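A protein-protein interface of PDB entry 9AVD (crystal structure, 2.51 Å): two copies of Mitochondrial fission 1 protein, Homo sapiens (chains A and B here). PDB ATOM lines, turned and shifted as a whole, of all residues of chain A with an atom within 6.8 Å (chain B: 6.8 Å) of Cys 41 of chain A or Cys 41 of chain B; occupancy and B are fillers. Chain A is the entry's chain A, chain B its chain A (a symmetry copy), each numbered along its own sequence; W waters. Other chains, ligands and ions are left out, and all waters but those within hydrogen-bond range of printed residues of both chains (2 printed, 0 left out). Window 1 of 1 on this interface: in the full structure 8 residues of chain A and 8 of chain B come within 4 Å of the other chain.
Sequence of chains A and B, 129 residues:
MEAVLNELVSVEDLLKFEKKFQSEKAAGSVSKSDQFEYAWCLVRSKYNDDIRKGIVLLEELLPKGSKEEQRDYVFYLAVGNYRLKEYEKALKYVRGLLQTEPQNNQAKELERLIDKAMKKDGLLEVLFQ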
ATOM      1  N   PHE A  36      21.099  19.214 -30.369  1.00  0.00           N
ATOM      2  CA  PHE A  36      21.633  17.913 -29.978  1.00  0.00           C
ATOM      3  C   PHE A  36      20.565  17.041 -29.322  1.00  0.00           C
ATOM      4  O   PHE A  36      20.242  15.949 -29.815  1.00  0.00           O
ATOM      5  CB  PHE A  36      22.820  18.103 -29.032  1.00  0.00           C
ATOM      6  CG  PHE A  36      23.417  16.816 -28.586  1.00  0.00           C
ATOM      7  CD1 PHE A  36      24.208  16.083 -29.452  1.00  0.00           C
ATOM      8  CD2 PHE A  36      23.143  16.303 -27.331  1.00  0.00           C
ATOM      9  CE1 PHE A  36      24.739  14.876 -29.070  1.00  0.00           C
ATOM     10  CE2 PHE A  36      23.678  15.093 -26.934  1.00  0.00           C
ATOM     11  CZ  PHE A  36      24.475  14.379 -27.806  1.00  0.00           C
ATOM     12  N   GLU A  37      20.029  17.501 -28.179  1.00  0.00           N
ATOM     13  CA  GLU A  37      18.929  16.838 -27.484  1.00  0.00           C
ATOM     14  C   GLU A  37      17.862  16.296 -28.435  1.00  0.00           C
ATOM     15  O   GLU A  37      17.494  15.119 -28.381  1.00  0.00           O
ATOM     16  CB  GLU A  37      18.297  17.823 -26.493  1.00  0.00           C
ATOM     17  CG  GLU A  37      19.182  18.236 -25.338  1.00  0.00           C
ATOM     18  CD  GLU A  37      19.735  17.048 -24.574  1.00  0.00           C
ATOM     19  OE1 GLU A  37      20.748  16.466 -25.013  1.00  0.00           O
ATOM     20  OE2 GLU A  37      19.145  16.678 -23.536  1.00  0.00           O
ATOM     21  N   TYR A  38      17.338  17.163 -29.303  1.00  0.00           N
ATOM     22  CA  TYR A  38      16.386  16.717 -30.309  1.00  0.00           C
ATOM     23  C   TYR A  38      16.952  15.568 -31.127  1.00  0.00           C
ATOM     24  O   TYR A  38      16.284  14.549 -31.346  1.00  0.00           O
ATOM     25  CB  TYR A  38      16.019  17.883 -31.219  1.00  0.00           C
ATOM     26  CG  TYR A  38      14.915  17.591 -32.205  1.00  0.00           C
ATOM     27  CD1 TYR A  38      13.874  16.723 -31.892  1.00  0.00           C
ATOM     28  CD2 TYR A  38      14.935  18.160 -33.475  1.00  0.00           C
ATOM     29  CE1 TYR A  38      12.866  16.455 -32.818  1.00  0.00           C
ATOM     30  CE2 TYR A  38      13.947  17.902 -34.390  1.00  0.00           C
ATOM     31  CZ  TYR A  38      12.914  17.049 -34.068  1.00  0.00           C
ATOM     32  OH  TYR A  38      11.929  16.789 -35.005  1.00  0.00           O
ATOM     33  N   ALA A  39      18.185  15.713 -31.596  1.00  0.00           N
ATOM     34  CA  ALA A  39      18.759  14.647 -32.401  1.00  0.00           C
ATOM     35  C   ALA A  39      19.127  13.459 -31.534  1.00  0.00           C
ATOM     36  O   ALA A  39      19.163  12.330 -32.026  1.00  0.00           O
ATOM     37  CB  ALA A  39      19.973  15.153 -33.182  1.00  0.00           C
ATOM     38  N   TRP A  40      19.389  13.681 -30.249  1.00  0.00           N
ATOM     39  CA  TRP A  40      19.636  12.546 -29.358  1.00  0.00           C
ATOM     40  C   TRP A  40      18.358  11.757 -29.133  1.00  0.00           C
ATOM     41  O   TRP A  40      18.350  10.526 -29.236  1.00  0.00           O
ATOM     42  CB  TRP A  40      20.212  13.015 -28.020  1.00  0.00           C
ATOM     43  CG  TRP A  40      20.518  11.911 -27.032  1.00  0.00           C
ATOM     44  CD1 TRP A  40      21.547  11.011 -27.099  1.00  0.00           C
ATOM     45  CD2 TRP A  40      19.824  11.631 -25.805  1.00  0.00           C
ATOM     46  NE1 TRP A  40      21.529  10.178 -26.000  1.00  0.00           N
ATOM     47  CE2 TRP A  40      20.483  10.537 -25.190  1.00  0.00           C
ATOM     48  CE3 TRP A  40      18.708  12.188 -25.174  1.00  0.00           C
ATOM     49  CZ2 TRP A  40      20.054   9.986 -23.972  1.00  0.00           C
ATOM     50  CZ3 TRP A  40      18.285  11.645 -23.964  1.00  0.00           C
ATOM     51  CH2 TRP A  40      18.957  10.551 -23.378  1.00  0.00           C
ATOM     52  N   CYS A  41      17.260  12.458 -28.839  1.00  0.00           N
ATOM     53  CA  CYS A  41      15.984  11.778 -28.677  1.00  0.00           C
ATOM     54  C   CYS A  41      15.561  11.119 -29.977  1.00  0.00           C
ATOM     55  O   CYS A  41      14.936  10.053 -29.964  1.00  0.00           O
ATOM     56  CB  CYS A  41      14.928  12.763 -28.179  1.00  0.00           C
ATOM     57  SG  CYS A  41      13.202  12.321 -28.605  1.00  0.00           S
ATOM     58  N   LEU A  42      15.920  11.717 -31.113  1.00  0.00           N
ATOM     59  CA  LEU A  42      15.554  11.130 -32.396  1.00  0.00           C
ATOM     60  C   LEU A  42      16.303   9.817 -32.627  1.00  0.00           C
ATOM     61  O   LEU A  42      15.692   8.768 -32.852  1.00  0.00           O
ATOM     62  CB  LEU A  42      15.813  12.126 -33.529  1.00  0.00           C
ATOM     63  CG  LEU A  42      14.694  13.116 -33.893  1.00  0.00           C
ATOM     64  CD1 LEU A  42      15.244  14.307 -34.676  1.00  0.00           C
ATOM     65  CD2 LEU A  42      13.564  12.474 -34.669  1.00  0.00           C
ATOM     66  N   VAL A  43      17.635   9.849 -32.541  1.00  0.00           N
ATOM     67  CA  VAL A  43      18.430   8.641 -32.741  1.00  0.00           C
ATOM     68  C   VAL A  43      18.063   7.530 -31.743  1.00  0.00           C
ATOM     69  O   VAL A  43      18.422   6.370 -31.950  1.00  0.00           O
ATOM     70  CB  VAL A  43      19.924   9.064 -32.715  1.00  0.00           C
ATOM     71  CG1 VAL A  43      20.842   7.966 -32.240  1.00  0.00           C
ATOM     72  CG2 VAL A  43      20.377   9.457 -34.096  1.00  0.00           C
ATOM     73  N   ARG A  44      17.342   7.845 -30.669  1.00  0.00           N
ATOM     74  CA  ARG A  44      16.891   6.835 -29.722  1.00  0.00           C
ATOM     75  C   ARG A  44      15.556   6.210 -30.107  1.00  0.00           C
ATOM     76  O   ARG A  44      15.143   5.249 -29.454  1.00  0.00           O
ATOM     77  CB  ARG A  44      16.740   7.426 -28.316  1.00  0.00           C
ATOM     78  CG  ARG A  44      18.020   7.783 -27.583  1.00  0.00           C
ATOM     79  CD  ARG A  44      17.803   8.960 -26.574  1.00  0.00           C
ATOM     80  NE  ARG A  44      17.186   8.569 -25.307  1.00  0.00           N
ATOM     81  CZ  ARG A  44      17.674   7.667 -24.466  1.00  0.00           C
ATOM     82  NH1 ARG A  44      18.790   6.997 -24.731  1.00  0.00           N
ATOM     83  NH2 ARG A  44      17.028   7.431 -23.324  1.00  0.00           N
ATOM     84  N   SER A  45      14.874   6.730 -31.131  1.00  0.00           N
ATOM     85  CA  SER A  45      13.487   6.355 -31.390  1.00  0.00           C
ATOM     86  C   SER A  45      13.383   4.943 -31.957  1.00  0.00           C
ATOM     87  O   SER A  45      14.328   4.390 -32.529  1.00  0.00           O
ATOM     88  CB  SER A  45      12.820   7.329 -32.362  1.00  0.00           C
ATOM     89  OG  SER A  45      12.787   6.808 -33.679  1.00  0.00           O
ATOM     90  N   LYS A  46      12.199   4.363 -31.799  1.00  0.00           N
ATOM     91  CA  LYS A  46      11.948   3.041 -32.350  1.00  0.00           C
ATOM     92  C   LYS A  46      11.695   3.066 -33.846  1.00  0.00           C
ATOM     93  O   LYS A  46      11.681   1.993 -34.468  1.00  0.00           O
ATOM     94  CB  LYS A  46      10.770   2.383 -31.626  1.00  0.00           C
ATOM     95  CG  LYS A  46       9.756   3.377 -31.114  1.00  0.00           C
ATOM     96  CD  LYS A  46       8.408   2.731 -30.823  1.00  0.00           C
ATOM     97  CE  LYS A  46       8.510   1.618 -29.808  1.00  0.00           C
ATOM     98  NZ  LYS A  46       7.169   1.162 -29.335  1.00  0.00           N
ATOM     99  N   ASP A  50      12.565   8.544 -37.843  1.00  0.00           N
ATOM    100  CA  ASP A  50      13.110   9.432 -36.827  1.00  0.00           C
ATOM    101  C   ASP A  50      14.626   9.267 -36.722  1.00  0.00           C
ATOM    102  O   ASP A  50      15.336  10.229 -36.417  1.00  0.00           O
ATOM    103  CB  ASP A  50      12.438   9.194 -35.468  1.00  0.00           C
ATOM    104  CG  ASP A  50      10.990   9.686 -35.428  1.00  0.00           C
ATOM    105  OD1 ASP A  50      10.287   9.526 -36.445  1.00  0.00           O
ATOM    106  OD2 ASP A  50      10.557  10.267 -34.401  1.00  0.00           O
ATOM    107  N   GLY A  54      17.326  12.123 -37.035  1.00  0.00           N
ATOM    108  CA  GLY A  54      18.279  12.311 -35.953  1.00  0.00           C
ATOM    109  C   GLY A  54      19.707  12.369 -36.459  1.00  0.00           C
ATOM    110  O   GLY A  54      20.512  13.177 -35.985  1.00  0.00           O
ATOM    111  N   ARG A  83      22.106   1.275 -35.760  1.00  0.00           N
ATOM    112  CA  ARG A  83      20.741   0.818 -35.533  1.00  0.00           C
ATOM    113  C   ARG A  83      19.976   0.657 -36.836  1.00  0.00           C
ATOM    114  O   ARG A  83      18.971  -0.060 -36.853  1.00  0.00           O
ATOM    115  CB  ARG A  83      19.997   1.777 -34.594  1.00  0.00           C
ATOM    116  CG  ARG A  83      20.407   1.582 -33.164  1.00  0.00           C
ATOM    117  CD  ARG A  83      19.230   1.541 -32.240  1.00  0.00           C
ATOM    118  NE  ARG A  83      18.695   2.876 -32.100  1.00  0.00           N
ATOM    119  CZ  ARG A  83      17.401   3.154 -32.032  1.00  0.00           C
ATOM    120  NH1 ARG A  83      16.491   2.196 -32.033  1.00  0.00           N
ATOM    121  NH2 ARG A  83      17.013   4.430 -31.966  1.00  0.00           N
ATOM    122  N   PHE B  36       6.964  21.418 -29.662  1.00  0.00           N
ATOM    123  CA  PHE B  36       6.060  20.304 -29.931  1.00  0.00           C
ATOM    124  C   PHE B  36       6.808  19.093 -30.482  1.00  0.00           C
ATOM    125  O   PHE B  36       6.797  18.007 -29.879  1.00  0.00           O
ATOM    126  CB  PHE B  36       4.969  20.746 -30.909  1.00  0.00           C
ATOM    127  CG  PHE B  36       4.008  19.659 -31.236  1.00  0.00           C
ATOM    128  CD1 PHE B  36       3.048  19.286 -30.314  1.00  0.00           C
ATOM    129  CD2 PHE B  36       4.097  18.967 -32.429  1.00  0.00           C
ATOM    130  CE1 PHE B  36       2.174  18.261 -30.583  1.00  0.00           C
ATOM    131  CE2 PHE B  36       3.219  17.940 -32.713  1.00  0.00           C
ATOM    132  CZ  PHE B  36       2.258  17.586 -31.788  1.00  0.00           C
ATOM    133  N   GLU B  37       7.439  19.256 -31.657  1.00  0.00           N
ATOM    134  CA  GLU B  37       8.280  18.230 -32.267  1.00  0.00           C
ATOM    135  C   GLU B  37       9.151  17.490 -31.251  1.00  0.00           C
ATOM    136  O   GLU B  37       9.149  16.257 -31.183  1.00  0.00           O
ATOM    137  CB  GLU B  37       9.163  18.878 -33.340  1.00  0.00           C
ATOM    138  CG  GLU B  37       8.424  19.422 -34.542  1.00  0.00           C
ATOM    139  CD  GLU B  37       7.530  18.384 -35.195  1.00  0.00           C
ATOM    140  OE1 GLU B  37       6.396  18.177 -34.715  1.00  0.00           O
ATOM    141  OE2 GLU B  37       7.967  17.754 -36.182  1.00  0.00           O
ATOM    142  N   TYR B  38       9.922  18.241 -30.465  1.00  0.00           N
ATOM    143  CA  TYR B  38      10.714  17.633 -29.405  1.00  0.00           C
ATOM    144  C   TYR B  38       9.842  16.791 -28.486  1.00  0.00           C
ATOM    145  O   TYR B  38      10.178  15.646 -28.158  1.00  0.00           O
ATOM    146  CB  TYR B  38      11.425  18.719 -28.609  1.00  0.00           C
ATOM    147  CG  TYR B  38      12.407  18.208 -27.582  1.00  0.00           C
ATOM    148  CD1 TYR B  38      13.136  17.043 -27.793  1.00  0.00           C
ATOM    149  CD2 TYR B  38      12.577  18.880 -26.374  1.00  0.00           C
ATOM    150  CE1 TYR B  38      14.031  16.578 -26.829  1.00  0.00           C
ATOM    151  CE2 TYR B  38      13.456  18.430 -25.424  1.00  0.00           C
ATOM    152  CZ  TYR B  38      14.182  17.279 -25.645  1.00  0.00           C
ATOM    153  OH  TYR B  38      15.058  16.830 -24.672  1.00  0.00           O
ATOM    154  N   ALA B  39       8.715  17.344 -28.052  1.00  0.00           N
ATOM    155  CA  ALA B  39       7.862  16.583 -27.156  1.00  0.00           C
ATOM    156  C   ALA B  39       7.142  15.480 -27.907  1.00  0.00           C
ATOM    157  O   ALA B  39       6.778  14.468 -27.307  1.00  0.00           O
ATOM    158  CB  ALA B  39       6.867  17.502 -26.447  1.00  0.00           C
ATOM    159  N   TRP B  40       6.940  15.643 -29.212  1.00  0.00           N
ATOM    160  CA  TRP B  40       6.351  14.552 -29.991  1.00  0.00           C
ATOM    161  C   TRP B  40       7.331  13.399 -30.117  1.00  0.00           C
ATOM    162  O   TRP B  40       6.972  12.238 -29.894  1.00  0.00           O
ATOM    163  CB  TRP B  40       5.921  15.037 -31.376  1.00  0.00           C
ATOM    164  CG  TRP B  40       5.284  13.984 -32.256  1.00  0.00           C
ATOM    165  CD1 TRP B  40       4.035  13.444 -32.116  1.00  0.00           C
ATOM    166  CD2 TRP B  40       5.844  13.391 -33.438  1.00  0.00           C
ATOM    167  NE1 TRP B  40       3.786  12.540 -33.127  1.00  0.00           N
ATOM    168  CE2 TRP B  40       4.879  12.488 -33.953  1.00  0.00           C
ATOM    169  CE3 TRP B  40       7.066  13.524 -34.104  1.00  0.00           C
ATOM    170  CZ2 TRP B  40       5.105  11.718 -35.104  1.00  0.00           C
ATOM    171  CZ3 TRP B  40       7.289  12.762 -35.249  1.00  0.00           C
ATOM    172  CH2 TRP B  40       6.312  11.867 -35.734  1.00  0.00           C
ATOM    173  N   CYS B  41       8.584  13.707 -30.462  1.00  0.00           N
ATOM    174  CA  CYS B  41       9.596  12.664 -30.537  1.00  0.00           C
ATOM    175  C   CYS B  41       9.822  12.040 -29.172  1.00  0.00           C
ATOM    176  O   CYS B  41      10.099  10.840 -29.071  1.00  0.00           O
ATOM    177  CB  CYS B  41      10.890  13.235 -31.113  1.00  0.00           C
ATOM    178  SG  CYS B  41      12.411  12.341 -30.621  1.00  0.00           S
ATOM    179  N   LEU B  42       9.675  12.826 -28.106  1.00  0.00           N
ATOM    180  CA  LEU B  42       9.868  12.286 -26.766  1.00  0.00           C
ATOM    181  C   LEU B  42       8.764  11.286 -26.419  1.00  0.00           C
ATOM    182  O   LEU B  42       9.038  10.130 -26.083  1.00  0.00           O
ATOM    183  CB  LEU B  42       9.935  13.420 -25.741  1.00  0.00           C
ATOM    184  CG  LEU B  42      11.305  14.062 -25.459  1.00  0.00           C
ATOM    185  CD1 LEU B  42      11.148  15.433 -24.806  1.00  0.00           C
ATOM    186  CD2 LEU B  42      12.203  13.190 -24.607  1.00  0.00           C
ATOM    187  N   VAL B  43       7.502  11.707 -26.527  1.00  0.00           N
ATOM    188  CA  VAL B  43       6.385  10.817 -26.222  1.00  0.00           C
ATOM    189  C   VAL B  43       6.388   9.555 -27.101  1.00  0.00           C
ATOM    190  O   VAL B  43       5.702   8.581 -26.786  1.00  0.00           O
ATOM    191  CB  VAL B  43       5.086  11.663 -26.312  1.00  0.00           C
ATOM    192  CG1 VAL B  43       3.874  10.849 -26.691  1.00  0.00           C
ATOM    193  CG2 VAL B  43       4.792  12.307 -24.984  1.00  0.00           C
ATOM    194  N   ARG B  44       7.155   9.533 -28.189  1.00  0.00           N
ATOM    195  CA  ARG B  44       7.269   8.346 -29.025  1.00  0.00           C
ATOM    196  C   ARG B  44       8.361   7.392 -28.560  1.00  0.00           C
ATOM    197  O   ARG B  44       8.458   6.291 -29.109  1.00  0.00           O
ATOM    198  CB  ARG B  44       7.568   8.724 -30.481  1.00  0.00           C
ATOM    199  CG  ARG B  44       6.442   9.373 -31.264  1.00  0.00           C
ATOM    200  CD  ARG B  44       6.986  10.326 -32.381  1.00  0.00           C
ATOM    201  NE  ARG B  44       7.438   9.647 -33.594  1.00  0.00           N
ATOM    202  CZ  ARG B  44       6.690   8.853 -34.349  1.00  0.00           C
ATOM    203  NH1 ARG B  44       5.430   8.577 -34.037  1.00  0.00           N
ATOM    204  NH2 ARG B  44       7.219   8.324 -35.452  1.00  0.00           N
ATOM    205  N   SER B  45       9.183   7.782 -27.582  1.00  0.00           N
ATOM    206  CA  SER B  45      10.398   7.036 -27.267  1.00  0.00           C
ATOM    207  C   SER B  45      10.084   5.721 -26.562  1.00  0.00           C
ATOM    208  O   SER B  45       9.025   5.535 -25.953  1.00  0.00           O
ATOM    209  CB  SER B  45      11.340   7.857 -26.386  1.00  0.00           C
ATOM    210  OG  SER B  45      11.235   7.482 -25.023  1.00  0.00           O
ATOM    211  N   LYS B  46      11.038   4.801 -26.645  1.00  0.00           N
ATOM    212  CA  LYS B  46      10.890   3.526 -25.963  1.00  0.00           C
ATOM    213  C   LYS B  46      11.161   3.621 -24.473  1.00  0.00           C
ATOM    214  O   LYS B  46      10.864   2.659 -23.749  1.00  0.00           O
ATOM    215  CB  LYS B  46      11.806   2.478 -26.600  1.00  0.00           C
ATOM    216  CG  LYS B  46      13.063   3.068 -27.192  1.00  0.00           C
ATOM    217  CD  LYS B  46      14.152   2.023 -27.399  1.00  0.00           C
ATOM    218  CE  LYS B  46      13.707   0.897 -28.301  1.00  0.00           C
ATOM    219  NZ  LYS B  46      14.843   0.017 -28.706  1.00  0.00           N
ATOM    220  N   ASP B  50      12.029   9.474 -21.047  1.00  0.00           N
ATOM    221  CA  ASP B  50      11.759  10.380 -22.154  1.00  0.00           C
ATOM    222  C   ASP B  50      10.262  10.665 -22.265  1.00  0.00           C
ATOM    223  O   ASP B  50       9.868  11.761 -22.674  1.00  0.00           O
ATOM    224  CB  ASP B  50      12.309   9.819 -23.472  1.00  0.00           C
ATOM    225  CG  ASP B  50      13.837   9.849 -23.539  1.00  0.00           C
ATOM    226  OD1 ASP B  50      14.475   9.587 -22.501  1.00  0.00           O
ATOM    227  OD2 ASP B  50      14.408  10.169 -24.612  1.00  0.00           O
ATOM    228  N   GLY B  54       8.544  14.214 -22.274  1.00  0.00           N
ATOM    229  CA  GLY B  54       7.675  14.571 -23.384  1.00  0.00           C
ATOM    230  C   GLY B  54       6.337  15.102 -22.909  1.00  0.00           C
ATOM    231  O   GLY B  54       5.804  16.063 -23.471  1.00  0.00           O
ATOM    232  N   ARG B  83       0.721   5.221 -22.550  1.00  0.00           N
ATOM    233  CA  ARG B  83       1.883   4.357 -22.710  1.00  0.00           C
ATOM    234  C   ARG B  83       2.585   4.103 -21.386  1.00  0.00           C
ATOM    235  O   ARG B  83       3.330   3.124 -21.283  1.00  0.00           O
ATOM    236  CB  ARG B  83       2.865   4.953 -23.727  1.00  0.00           C
ATOM    237  CG  ARG B  83       2.395   4.750 -25.137  1.00  0.00           C
ATOM    238  CD  ARG B  83       3.492   4.268 -26.035  1.00  0.00           C
ATOM    239  NE  ARG B  83       4.400   5.362 -26.297  1.00  0.00           N
ATOM    240  CZ  ARG B  83       5.716   5.232 -26.372  1.00  0.00           C
ATOM    241  NH1 ARG B  83       6.297   4.050 -26.263  1.00  0.00           N
ATOM    242  NH2 ARG B  83       6.466   6.321 -26.558  1.00  0.00           N
HETATM  243  O   HOH W   1      10.486   6.350 -30.465  1.00  0.00           O
HETATM  244  O   HOH W   2      13.246   6.043 -28.142  1.00  0.00           O
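SG of Cys 41 of chain B forms a disulfide with SG of Cys 41 of chain A, 2.2 Å away.
N of Leu 42 of chain B is in hydrogen-bond range of SG of Cys 41 of chain A, 3.6 Å away.
N of Leu 42 of chain A lies within hydrogen-bond range of SG of Cys 41 of chain B, at 3.6 Å.
OD2 of Asp 50 of chain B lies within salt-bridge range of NE of Arg 44 of chain A (3.3 Å).
The side-chain carboxylate (OD2) of Asp 50 of chain A lies within salt-bridge range of the guanidinium group (NE) of Arg 44 of chain B (3.3 Å).
The backbone carbonyl oxygen of Arg 44 of chain A sits close to the guanidinium group of Arg 83 of chain A (3.2 Å).
The backbone carbonyl oxygen of Arg 44 of chain B lies close to the guanidinium group of Arg 83 of chain B (3.2 Å).
Among the printed residues, merely in contact across the chains: Lys 46 of chain A with Arg 44 of chain B, Arg 44 of chain A with Lys 46 of chain B, Tyr 38 of chain A with Glu 37 of chain B and Glu 37 of chain A with Tyr 38 of chain B.
Cys 41 of chain A touches just these residues of chain B: Cys 41 and Leu 42.
Of the printed residues of chain A, Tyr 38 of chain B touches Glu 37 (3.8 Å).
Cys 41 of chain B touches two residues of chain A.
Of the printed residues of chain A, Arg 44 of chain B touches Lys 46 and Asp 50.
Ser 45 of chain B touches none of the printed residues of chain A.
Gly 54 of chain B touches none of the printed residues of chain A.
The nearest residue of chain A that does not touch Cys 41 of chain B is Tyr 38 of chain A (4.1 Å).
Of the 14 printed residues of chain B, 7 touch a printed residue of chain A.
Printed residues of chain B that touch a printed residue of chain A: Glu 37, Tyr 38, Cys 41, Leu 42, Arg 44, Lys 46 and Asp 50.
Hydrophobic or aromatic side chains of chain B that line the printed part of chain A: Tyr 38.
Printed residues of chain A that touch a printed residue of chain B: Glu 37, Tyr 38, Cys 41, Leu 42, Arg 44, Lys 46 and Asp 50.
Hydrophobic or aromatic side chains of chain A that line the printed part of chain B: Tyr 38.
Among the printed residues, 9 pairs touch across the chains.
Among the printed residues, Asp or Glu carboxylates within 4 Å of a Lys or Arg side-chain nitrogen of the other chain: Arg 44 of chain A with Asp 50 of chain B (3.3 Å) and Asp 50 of chain A with Arg 44 of chain B (3.3 Å).
Glu 37 of chain A touches Tyr 38 of chain B, and with the chains exchanged Tyr 38 of chain A touches Glu 37 of chain B.
Cys 41 of chain B touches its own counterpart, Cys 41 of chain A.
Cys 41 of chain A touches Leu 42 of chain B, and with the chains exchanged Leu 42 of chain A touches Cys 41 of chain B.
Arg 44 of chain A touches Lys 46 of chain B, and with the chains exchanged Lys 46 of chain A touches Arg 44 of chain B.
14 positions are printed for both chains.
Of the 9 pairs that touch across the chains among the printed residues, 9 have their exchanged pair printed and touching as well.
Water W2 lies within hydrogen-bond range of O of Arg 44 of chain A (2.4 Å), N of Lys 46 of chain B (2.9 Å) and N of Ser 45 of chain A (3.5 Å).
Water W1 lies within hydrogen-bond range of O of Arg 44 of chain B (2.4 Å), N of Lys 46 of chain A (2.9 Å) and N of Ser 45 of chain B (3.5 Å).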
